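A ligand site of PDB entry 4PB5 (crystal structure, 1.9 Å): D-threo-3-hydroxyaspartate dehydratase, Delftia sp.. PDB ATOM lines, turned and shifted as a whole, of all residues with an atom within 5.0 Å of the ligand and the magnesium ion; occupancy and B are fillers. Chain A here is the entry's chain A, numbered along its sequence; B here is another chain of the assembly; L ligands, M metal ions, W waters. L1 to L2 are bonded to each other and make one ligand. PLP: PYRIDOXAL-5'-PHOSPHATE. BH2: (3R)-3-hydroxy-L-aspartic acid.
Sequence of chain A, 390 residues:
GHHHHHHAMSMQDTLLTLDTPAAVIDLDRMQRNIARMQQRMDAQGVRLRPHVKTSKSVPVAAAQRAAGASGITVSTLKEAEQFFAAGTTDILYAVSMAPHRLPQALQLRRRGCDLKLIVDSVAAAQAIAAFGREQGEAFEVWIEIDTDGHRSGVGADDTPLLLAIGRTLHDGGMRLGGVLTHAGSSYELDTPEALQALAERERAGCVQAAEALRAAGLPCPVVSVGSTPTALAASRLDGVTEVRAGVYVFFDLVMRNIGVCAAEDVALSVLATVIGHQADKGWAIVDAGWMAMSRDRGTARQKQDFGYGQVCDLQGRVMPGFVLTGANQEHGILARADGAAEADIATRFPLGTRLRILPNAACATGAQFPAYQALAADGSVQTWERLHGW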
ATOM      1  N   HIS A  51     -23.434  30.364   2.282  1.00  0.00           N
ATOM      2  CA  HIS A  51     -23.753  30.323   3.682  1.00  0.00           C
ATOM      3  C   HIS A  51     -22.719  31.155   4.455  1.00  0.00           C
ATOM      4  O   HIS A  51     -21.532  30.736   4.630  1.00  0.00           O
ATOM      5  CB  HIS A  51     -23.821  28.893   4.254  1.00  0.00           C
ATOM      6  CG  HIS A  51     -24.782  28.860   5.415  1.00  0.00           C
ATOM      7  ND1 HIS A  51     -24.755  29.842   6.362  1.00  0.00           N
ATOM      8  CD2 HIS A  51     -25.773  28.019   5.754  1.00  0.00           C
ATOM      9  CE1 HIS A  51     -25.768  29.610   7.222  1.00  0.00           C
ATOM     10  NE2 HIS A  51     -26.370  28.495   6.847  1.00  0.00           N
ATOM     11  N   LYS A  53     -22.536  31.840   7.500  1.00  0.00           N
ATOM     12  CA  LYS A  53     -22.168  31.414   8.875  1.00  0.00           C
ATOM     13  C   LYS A  53     -20.651  31.063   9.024  1.00  0.00           C
ATOM     14  O   LYS A  53     -20.156  31.082  10.113  1.00  0.00           O
ATOM     15  CB  LYS A  53     -23.020  30.258   9.361  1.00  0.00           C
ATOM     16  CG  LYS A  53     -22.627  28.922   8.717  1.00  0.00           C
ATOM     17  CD  LYS A  53     -23.573  27.880   9.310  1.00  0.00           C
ATOM     18  CE  LYS A  53     -23.377  26.542   8.618  1.00  0.00           C
ATOM     19  NZ  LYS A  53     -21.928  26.156   8.885  1.00  0.00           N
ATOM     20  N   THR A  54     -19.970  30.785   7.925  1.00  0.00           N
ATOM     21  CA  THR A  54     -18.545  30.401   8.045  1.00  0.00           C
ATOM     22  C   THR A  54     -17.702  31.625   8.486  1.00  0.00           C
ATOM     23  O   THR A  54     -16.817  31.474   9.343  1.00  0.00           O
ATOM     24  CB  THR A  54     -18.069  29.871   6.647  1.00  0.00           C
ATOM     25  OG1 THR A  54     -18.752  28.605   6.435  1.00  0.00           O
ATOM     26  CG2 THR A  54     -16.545  29.583   6.720  1.00  0.00           C
ATOM     27  N   THR A  73     -27.256  32.828   2.784  1.00  0.00           N
ATOM     28  CA  THR A  73     -27.948  31.989   3.740  1.00  0.00           C
ATOM     29  C   THR A  73     -27.331  32.380   5.078  1.00  0.00           C
ATOM     30  O   THR A  73     -26.110  32.607   5.133  1.00  0.00           O
ATOM     31  CB  THR A  73     -27.648  30.507   3.510  1.00  0.00           C
ATOM     32  OG1 THR A  73     -27.891  30.155   2.120  1.00  0.00           O
ATOM     33  CG2 THR A  73     -28.620  29.609   4.434  1.00  0.00           C
ATOM     34  N   ALA A  94     -31.742  29.658   7.440  1.00  0.00           N
ATOM     35  CA  ALA A  94     -31.962  28.247   7.179  1.00  0.00           C
ATOM     36  C   ALA A  94     -31.812  27.406   8.444  1.00  0.00           C
ATOM     37  O   ALA A  94     -31.049  26.448   8.468  1.00  0.00           O
ATOM     38  CB  ALA A  94     -30.978  27.780   6.042  1.00  0.00           C
ATOM     39  N   ARG A 151     -30.302  15.330   9.913  1.00  0.00           N
ATOM     40  CA  ARG A 151     -30.695  16.432  10.830  1.00  0.00           C
ATOM     41  C   ARG A 151     -32.215  16.710  10.653  1.00  0.00           C
ATOM     42  O   ARG A 151     -33.005  15.781  10.846  1.00  0.00           O
ATOM     43  CB  ARG A 151     -29.847  17.679  10.537  1.00  0.00           C
ATOM     44  CG  ARG A 151     -29.771  18.764  11.643  1.00  0.00           C
ATOM     45  CD  ARG A 151     -28.733  19.818  11.273  1.00  0.00           C
ATOM     46  NE  ARG A 151     -29.128  20.715  10.173  1.00  0.00           N
ATOM     47  CZ  ARG A 151     -28.232  21.515   9.537  1.00  0.00           C
ATOM     48  NH1 ARG A 151     -26.927  21.439   9.889  1.00  0.00           N
ATOM     49  NH2 ARG A 151     -28.628  22.431   8.616  1.00  0.00           N
ATOM     50  N   LEU A 180     -35.932  23.091   0.455  1.00  0.00           N
ATOM     51  CA  LEU A 180     -34.477  23.112   0.555  1.00  0.00           C
ATOM     52  C   LEU A 180     -34.030  21.865   1.264  1.00  0.00           C
ATOM     53  O   LEU A 180     -34.804  21.283   2.054  1.00  0.00           O
ATOM     54  CB  LEU A 180     -33.935  24.351   1.303  1.00  0.00           C
ATOM     55  CG  LEU A 180     -33.982  24.287   2.823  1.00  0.00           C
ATOM     56  CD1 LEU A 180     -32.952  25.325   3.345  1.00  0.00           C
ATOM     57  CD2 LEU A 180     -35.433  24.584   3.243  1.00  0.00           C
ATOM     58  N   HIS A 182     -30.242  19.969   3.089  1.00  0.00           N
ATOM     59  CA  HIS A 182     -28.813  20.011   3.316  1.00  0.00           C
ATOM     60  C   HIS A 182     -28.292  18.594   3.596  1.00  0.00           C
ATOM     61  O   HIS A 182     -28.681  17.980   4.610  1.00  0.00           O
ATOM     62  CB  HIS A 182     -28.505  20.961   4.482  1.00  0.00           C
ATOM     63  CG  HIS A 182     -27.089  20.831   4.994  1.00  0.00           C
ATOM     64  ND1 HIS A 182     -26.016  21.331   4.327  1.00  0.00           N
ATOM     65  CD2 HIS A 182     -26.615  20.347   6.209  1.00  0.00           C
ATOM     66  CE1 HIS A 182     -24.909  21.119   5.087  1.00  0.00           C
ATOM     67  NE2 HIS A 182     -25.294  20.488   6.220  1.00  0.00           N
ATOM     68  N   TYR A 187     -20.246  14.857   5.187  1.00  0.00           N
ATOM     69  CA  TYR A 187     -19.069  15.017   6.071  1.00  0.00           C
ATOM     70  C   TYR A 187     -18.496  13.695   6.533  1.00  0.00           C
ATOM     71  O   TYR A 187     -17.350  13.653   6.964  1.00  0.00           O
ATOM     72  CB  TYR A 187     -19.346  15.961   7.296  1.00  0.00           C
ATOM     73  CG  TYR A 187     -19.382  17.432   6.918  1.00  0.00           C
ATOM     74  CD1 TYR A 187     -20.339  17.965   6.007  1.00  0.00           C
ATOM     75  CD2 TYR A 187     -18.418  18.293   7.451  1.00  0.00           C
ATOM     76  CE1 TYR A 187     -20.378  19.363   5.697  1.00  0.00           C
ATOM     77  CE2 TYR A 187     -18.400  19.655   7.143  1.00  0.00           C
ATOM     78  CZ  TYR A 187     -19.382  20.178   6.245  1.00  0.00           C
ATOM     79  OH  TYR A 187     -19.302  21.523   5.918  1.00  0.00           O
ATOM     80  N   GLY A 226     -27.560  21.726  -0.792  1.00  0.00           N
ATOM     81  CA  GLY A 226     -26.120  21.886  -0.793  1.00  0.00           C
ATOM     82  C   GLY A 226     -25.410  21.681   0.559  1.00  0.00           C
ATOM     83  O   GLY A 226     -25.998  21.948   1.671  1.00  0.00           O
ATOM     84  N   SER A 227     -24.153  21.247   0.442  1.00  0.00           N
ATOM     85  CA  SER A 227     -23.166  21.341   1.529  1.00  0.00           C
ATOM     86  C   SER A 227     -21.918  21.616   0.686  1.00  0.00           C
ATOM     87  O   SER A 227     -21.995  21.438  -0.541  1.00  0.00           O
ATOM     88  CB  SER A 227     -23.033  20.020   2.281  1.00  0.00           C
ATOM     89  OG  SER A 227     -22.653  18.988   1.376  1.00  0.00           O
ATOM     90  N   THR A 228     -20.796  22.022   1.266  1.00  0.00           N
ATOM     91  CA  THR A 228     -19.626  22.246   0.388  1.00  0.00           C
ATOM     92  C   THR A 228     -19.231  20.959  -0.376  1.00  0.00           C
ATOM     93  O   THR A 228     -18.976  21.013  -1.597  1.00  0.00           O
ATOM     94  CB  THR A 228     -18.459  22.901   1.179  1.00  0.00           C
ATOM     95  OG1 THR A 228     -18.790  24.276   1.384  1.00  0.00           O
ATOM     96  CG2 THR A 228     -17.041  22.760   0.458  1.00  0.00           C
ATOM     97  N   PRO A 229     -19.141  19.799   0.317  1.00  0.00           N
ATOM     98  CA  PRO A 229     -18.735  18.606  -0.418  1.00  0.00           C
ATOM     99  C   PRO A 229     -19.674  18.229  -1.542  1.00  0.00           C
ATOM    100  O   PRO A 229     -19.196  17.879  -2.675  1.00  0.00           O
ATOM    101  CB  PRO A 229     -18.697  17.482   0.658  1.00  0.00           C
ATOM    102  CG  PRO A 229     -18.345  18.283   1.904  1.00  0.00           C
ATOM    103  CD  PRO A 229     -19.203  19.547   1.793  1.00  0.00           C
ATOM    104  N   ARG A 244     -26.440  25.983  -1.872  1.00  0.00           N
ATOM    105  CA  ARG A 244     -25.929  26.721  -0.692  1.00  0.00           C
ATOM    106  C   ARG A 244     -24.624  26.059  -0.244  1.00  0.00           C
ATOM    107  O   ARG A 244     -24.552  24.836  -0.127  1.00  0.00           O
ATOM    108  CB  ARG A 244     -26.922  26.655   0.481  1.00  0.00           C
ATOM    109  CG  ARG A 244     -28.345  27.191   0.085  1.00  0.00           C
ATOM    110  CD  ARG A 244     -29.335  27.111   1.314  1.00  0.00           C
ATOM    111  NE  ARG A 244     -29.069  25.890   2.042  1.00  0.00           N
ATOM    112  CZ  ARG A 244     -29.447  24.653   1.650  1.00  0.00           C
ATOM    113  NH1 ARG A 244     -30.234  24.493   0.531  1.00  0.00           N
ATOM    114  NH2 ARG A 244     -28.950  23.557   2.312  1.00  0.00           N
ATOM    115  N   ALA A 245     -23.592  26.831  -0.032  1.00  0.00           N
ATOM    116  CA  ALA A 245     -22.279  26.306   0.463  1.00  0.00           C
ATOM    117  C   ALA A 245     -21.638  27.404   1.225  1.00  0.00           C
ATOM    118  O   ALA A 245     -21.765  28.556   0.860  1.00  0.00           O
ATOM    119  CB  ALA A 245     -21.326  25.875  -0.688  1.00  0.00           C
ATOM    120  N   GLY A 246     -20.877  27.059   2.266  1.00  0.00           N
ATOM    121  CA  GLY A 246     -20.290  28.128   3.075  1.00  0.00           C
ATOM    122  C   GLY A 246     -18.814  27.859   3.374  1.00  0.00           C
ATOM    123  O   GLY A 246     -18.003  28.797   3.240  1.00  0.00           O
ATOM    124  N   VAL A 247     -18.461  26.649   3.845  1.00  0.00           N
ATOM    125  CA  VAL A 247     -17.068  26.501   4.403  1.00  0.00           C
ATOM    126  C   VAL A 247     -15.970  26.602   3.285  1.00  0.00           C
ATOM    127  O   VAL A 247     -14.844  27.027   3.568  1.00  0.00           O
ATOM    128  CB  VAL A 247     -16.934  25.196   5.207  1.00  0.00           C
ATOM    129  CG1 VAL A 247     -16.988  23.934   4.314  1.00  0.00           C
ATOM    130  CG2 VAL A 247     -15.590  25.168   5.984  1.00  0.00           C
ATOM    131  N   TYR A 248     -16.383  26.351   2.040  1.00  0.00           N
ATOM    132  CA  TYR A 248     -15.456  26.412   0.876  1.00  0.00           C
ATOM    133  C   TYR A 248     -14.748  27.747   0.772  1.00  0.00           C
ATOM    134  O   TYR A 248     -13.692  27.830   0.183  1.00  0.00           O
ATOM    135  CB  TYR A 248     -16.307  26.214  -0.443  1.00  0.00           C
ATOM    136  CG  TYR A 248     -17.005  27.509  -0.873  1.00  0.00           C
ATOM    137  CD1 TYR A 248     -18.264  27.877  -0.326  1.00  0.00           C
ATOM    138  CD2 TYR A 248     -16.372  28.428  -1.781  1.00  0.00           C
ATOM    139  CE1 TYR A 248     -18.860  29.088  -0.681  1.00  0.00           C
ATOM    140  CE2 TYR A 248     -16.980  29.629  -2.128  1.00  0.00           C
ATOM    141  CZ  TYR A 248     -18.245  29.918  -1.567  1.00  0.00           C
ATOM    142  OH  TYR A 248     -18.860  31.090  -1.883  1.00  0.00           O
ATOM    143  N   MET A 255     -12.313  19.321   5.285  1.00  0.00           N
ATOM    144  CA  MET A 255     -12.641  19.318   3.829  1.00  0.00           C
ATOM    145  C   MET A 255     -11.529  18.632   3.083  1.00  0.00           C
ATOM    146  O   MET A 255     -11.792  17.898   2.109  1.00  0.00           O
ATOM    147  CB  MET A 255     -12.852  20.769   3.316  1.00  0.00           C
ATOM    148  CG  MET A 255     -14.173  21.403   3.853  1.00  0.00           C
ATOM    149  SD  MET A 255     -15.641  20.513   3.186  1.00  0.00           S
ATOM    150  CE  MET A 255     -16.412  20.165   4.747  1.00  0.00           C
ATOM    151  N   CYS A 363     -15.272  27.018  10.277  1.00  0.00           N
ATOM    152  CA  CYS A 363     -16.448  27.715  10.893  1.00  0.00           C
ATOM    153  C   CYS A 363     -16.231  27.816  12.419  1.00  0.00           C
ATOM    154  O   CYS A 363     -16.643  28.820  12.996  1.00  0.00           O
ATOM    155  CB  CYS A 363     -17.678  26.810  10.747  1.00  0.00           C
ATOM    156  SG  CYS A 363     -18.085  26.569   8.930  1.00  0.00           S
ATOM    157  N   TRP B 290     -23.322  23.331  18.504  1.00  0.00           N
ATOM    158  CA  TRP B 290     -21.982  23.505  19.094  1.00  0.00           C
ATOM    159  C   TRP B 290     -21.541  24.924  19.144  1.00  0.00           C
ATOM    160  O   TRP B 290     -20.619  25.282  19.923  1.00  0.00           O
ATOM    161  CB  TRP B 290     -20.897  22.579  18.484  1.00  0.00           C
ATOM    162  CG  TRP B 290     -20.658  22.838  17.018  1.00  0.00           C
ATOM    163  CD1 TRP B 290     -21.073  22.040  15.952  1.00  0.00           C
ATOM    164  CD2 TRP B 290     -19.975  23.976  16.409  1.00  0.00           C
ATOM    165  NE1 TRP B 290     -20.637  22.579  14.768  1.00  0.00           N
ATOM    166  CE2 TRP B 290     -20.014  23.767  14.964  1.00  0.00           C
ATOM    167  CE3 TRP B 290     -19.306  25.111  16.923  1.00  0.00           C
ATOM    168  CZ2 TRP B 290     -19.431  24.682  14.050  1.00  0.00           C
ATOM    169  CZ3 TRP B 290     -18.720  26.024  16.000  1.00  0.00           C
ATOM    170  CH2 TRP B 290     -18.796  25.798  14.607  1.00  0.00           C
ATOM    171  N   ASN B 328     -24.856  20.130  15.454  1.00  0.00           N
ATOM    172  CA  ASN B 328     -24.266  20.885  14.363  1.00  0.00           C
ATOM    173  C   ASN B 328     -24.170  22.345  14.809  1.00  0.00           C
ATOM    174  O   ASN B 328     -24.313  22.639  15.981  1.00  0.00           O
ATOM    175  CB  ASN B 328     -25.086  20.722  13.063  1.00  0.00           C
ATOM    176  CG  ASN B 328     -25.104  19.236  12.582  1.00  0.00           C
ATOM    177  OD1 ASN B 328     -26.092  18.748  12.258  1.00  0.00           O
ATOM    178  ND2 ASN B 328     -24.013  18.539  12.702  1.00  0.00           N
ATOM    179  N   GLN B 329     -23.857  23.230  13.854  1.00  0.00           N
ATOM    180  CA  GLN B 329     -23.436  24.585  14.264  1.00  0.00           C
ATOM    181  C   GLN B 329     -24.535  25.254  15.133  1.00  0.00           C
ATOM    182  O   GLN B 329     -24.238  25.673  16.249  1.00  0.00           O
ATOM    183  CB  GLN B 329     -23.117  25.469  13.014  1.00  0.00           C
ATOM    184  CG  GLN B 329     -22.333  26.713  13.496  1.00  0.00           C
ATOM    185  CD  GLN B 329     -21.564  27.348  12.360  1.00  0.00           C
ATOM    186  OE1 GLN B 329     -20.982  26.635  11.524  1.00  0.00           O
ATOM    187  NE2 GLN B 329     -21.564  28.713  12.290  1.00  0.00           N
ATOM    188  N   GLU B 330     -25.749  25.292  14.624  1.00  0.00           N
ATOM    189  CA  GLU B 330     -26.869  25.970  15.304  1.00  0.00           C
ATOM    190  C   GLU B 330     -27.989  24.986  15.640  1.00  0.00           C
ATOM    191  O   GLU B 330     -29.143  25.423  15.889  1.00  0.00           O
ATOM    192  CB  GLU B 330     -27.392  27.163  14.434  1.00  0.00           C
ATOM    193  CG  GLU B 330     -26.322  28.284  14.379  1.00  0.00           C
ATOM    194  CD  GLU B 330     -26.050  28.979  15.742  1.00  0.00           C
ATOM    195  OE1 GLU B 330     -26.874  28.955  16.686  1.00  0.00           O
ATOM    196  OE2 GLU B 330     -24.990  29.593  15.870  1.00  0.00           O
ATOM    197  N   HIS B 331     -27.742  23.683  15.527  1.00  0.00           N
ATOM    198  CA  HIS B 331     -28.792  22.668  15.794  1.00  0.00           C
ATOM    199  C   HIS B 331     -28.233  21.694  16.788  1.00  0.00           C
ATOM    200  O   HIS B 331     -27.141  21.163  16.567  1.00  0.00           O
ATOM    201  CB  HIS B 331     -29.140  21.827  14.552  1.00  0.00           C
ATOM    202  CG  HIS B 331     -29.740  22.568  13.391  1.00  0.00           C
ATOM    203  ND1 HIS B 331     -28.993  23.282  12.539  1.00  0.00           N
ATOM    204  CD2 HIS B 331     -31.055  22.598  12.901  1.00  0.00           C
ATOM    205  CE1 HIS B 331     -29.790  23.770  11.550  1.00  0.00           C
ATOM    206  NE2 HIS B 331     -31.048  23.337  11.774  1.00  0.00           N
HETATM  207  N1  PLP L   1     -27.103  24.894   4.186  1.00  0.00           N
HETATM  208  C2  PLP L   1     -27.465  24.574   5.475  1.00  0.00           C
HETATM  209  C2A PLP L   1     -28.884  24.486   5.946  1.00  0.00           C
HETATM  210  C3  PLP L   1     -26.410  24.360   6.450  1.00  0.00           C
HETATM  211  O3  PLP L   1     -26.760  24.025   7.681  1.00  0.00           O
HETATM  212  C4  PLP L   1     -25.018  24.441   5.938  1.00  0.00           C
HETATM  213  C4A PLP L   1     -23.872  24.171   6.790  1.00  0.00           C
HETATM  214  C5  PLP L   1     -24.726  24.795   4.558  1.00  0.00           C
HETATM  215  C6  PLP L   1     -25.839  25.009   3.722  1.00  0.00           C
HETATM  216  C5A PLP L   1     -23.301  24.995   4.091  1.00  0.00           C
HETATM  217  O4P PLP L   1     -22.626  23.726   4.117  1.00  0.00           O
HETATM  218  P   PLP L   1     -21.045  23.684   4.277  1.00  0.00           P
HETATM  219  O1P PLP L   1     -20.586  24.739   3.361  1.00  0.00           O
HETATM  220  O2P PLP L   1     -20.662  22.233   3.978  1.00  0.00           O
HETATM  221  O3P PLP L   1     -20.770  24.168   5.646  1.00  0.00           O
HETATM  222  C   BH2 L   2     -23.553  22.829  10.312  1.00  0.00           C
HETATM  223  N   BH2 L   2     -24.107  23.314   8.036  1.00  0.00           N
HETATM  224  O   BH2 L   2     -22.689  22.634  11.154  1.00  0.00           O
HETATM  225  CA  BH2 L   2     -23.361  22.429   8.856  1.00  0.00           C
HETATM  226  CB  BH2 L   2     -21.960  22.201   8.275  1.00  0.00           C
HETATM  227  OB  BH2 L   2     -21.340  23.494   8.133  1.00  0.00           O
HETATM  228  CG  BH2 L   2     -21.156  21.203   9.124  1.00  0.00           C
HETATM  229  OD1 BH2 L   2     -21.737  20.141   9.316  1.00  0.00           O
HETATM  230  OD2 BH2 L   2     -19.983  21.452   9.617  1.00  0.00           O
HETATM  231  OXT BH2 L   2     -24.685  23.194  10.617  1.00  0.00           O
HETATM  232 MG    MG M   1     -19.341  23.317   9.323  1.00  0.00          MG
HETATM  233  O   HOH W   1     -24.576  19.786   9.059  1.00  0.00           O
HETATM  234  O   HOH W   2     -20.887  26.839   6.267  1.00  0.00           O
HETATM  235  O   HOH W   3     -20.398  23.931  10.955  1.00  0.00           O
HETATM  236  O   HOH W   4     -26.723  25.947   9.858  1.00  0.00           O
HETATM  237  O   HOH W   5     -19.210  19.496  10.877  1.00  0.00           O
HETATM  238  O   HOH W   6     -18.238  22.726   7.673  1.00  0.00           O
HETATM  239  O   HOH W   7     -17.774  23.049  10.686  1.00  0.00           O
HETATM  240  O   HOH W   8     -26.507  24.307  12.089  1.00  0.00           O
HETATM  241  O   HOH W   9     -21.348  20.781  12.427  1.00  0.00           O
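The side-chain hydroxyl (OG1) of Thr 228 lies within hydrogen-bond range of an oxygen (O1P) of PLP L1 (2.7 Å).
The side-chain hydroxyl of Tyr 187 is in hydrogen-bond range of an oxygen (O2P) of PLP L1, 2.5 Å away.
The backbone NH (N) of Gln 329 of chain B sits at hydrogen-bond distance from an oxygen (O) of BH2 L2 (3.0 Å).
An oxygen (O2P) of PLP L1 lies within hydrogen-bond range of the backbone NH (N) of Thr 228, 2.7 Å away.
NH2 of Arg 244 is in hydrogen-bond range of N1 of PLP L1 (3.0 Å).
OXT of BH2 L2 is in salt-bridge range of NH1 of Arg 151, at 2.9 Å.
NZ of Lys 53 is in salt-bridge range of O3P of PLP L1 (3.97 Å).
An oxygen (O1P) of PLP L1 lies within hydrogen-bond range of the backbone NH (N) of Val 247 (2.9 Å).
An oxygen (O1P) of PLP L1 is in hydrogen-bond range of the backbone NH (N) of Gly 246 (2.6 Å).
The backbone carbonyl oxygen of Gly 226 lies within hydrogen-bond range of a ring nitrogen (ND1) of His 182 (2.7 Å).
The backbone carbonyl oxygen (O) of Gly 226 lies within hydrogen-bond range of the guanidinium group (NH2) of Arg 244, 3.4 Å away.
The side-chain hydroxyl (OG1) of Thr 54 sits at hydrogen-bond distance from the backbone NH (N) of Val 247.
The backbone carbonyl oxygen of Gly 246 sits close to the side-chain hydroxyl of Thr 54 (3.3 Å).
NE of Arg 151 lies close to ND1 of His 331 of chain B (3.5 Å).
A ring nitrogen (ND1) of His 51 sits at hydrogen-bond distance from the backbone carbonyl oxygen (O) of Thr 73, 3.3 Å away.
The backbone NH (N) of Tyr 248 is in hydrogen-bond range of the side-chain hydroxyl (OG1) of Thr 228 (3.2 Å).
The backbone NH (N) of Trp 290 of chain B sits at hydrogen-bond distance from the backbone carbonyl oxygen (O) of Gln 329 of chain B, at 3.4 Å.
Merely in contact with the ligand: His 51 (3.6 Å), Ala 94 (3.9 Å), His 182 (3.4 Å), Gly 226 (3.7 Å), Ser 227 (3.6 Å), Pro 229 (3.8 Å), Ala 245 (3.6 Å) and Asn 328 of chain B (3.5 Å).
Hydrophobic or aromatic side chains within 4 Å of the ligand: His 51, Ala 94, His 182, Tyr 187, Pro 229 and Val 247.
The nearest printed residue that does not touch the ligand is Trp 290 of chain B (4.2 Å).
Lys 53 touches the magnesium ion.
Tyr 187 touches the magnesium ion (OH to MG, 3.8 Å).
SG of Cys 363 touches the magnesium ion, 3.5 Å away.
The magnesium ion is bound by OD2 of BH2 L2 (2.0 Å), water W3 (2.0 Å), water W6 (2.1 Å), water W7 (2.1 Å) and OB of BH2 L2 (2.3 Å).
The magnesium ion has five donor atoms within binding distance.
Water W3 lies within hydrogen-bond range of an oxygen (O) of BH2 L2, the side-chain amide oxygen (OE1) of Gln 329 of chain B and the side-chain amino group (NZ) of Lys 53.
Water W8 lies within hydrogen-bond range of OXT of BH2 L2, ND1 of His 331 of chain B, N of Glu 330 of chain B and N of Gln 329 of chain B.
Water W9 lies within hydrogen-bond range of an oxygen (O) of BH2 L2 (2.6 Å), the indole nitrogen (NE1) of Trp 290 of chain B (3.0 Å) and the side-chain amide nitrogen (ND2) of Asn 328 of chain B (3.5 Å).
Water W2 lies within hydrogen-bond range of an oxygen (O3P) of PLP L1, the side-chain hydroxyl (OG1) of Thr 54, the side-chain amino group (NZ) of Lys 53 and the backbone NH (N) of Val 247.
Water W1 lies within hydrogen-bond range of OD1 of BH2 L2, NH1 of Arg 151 and NE2 of His 182.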
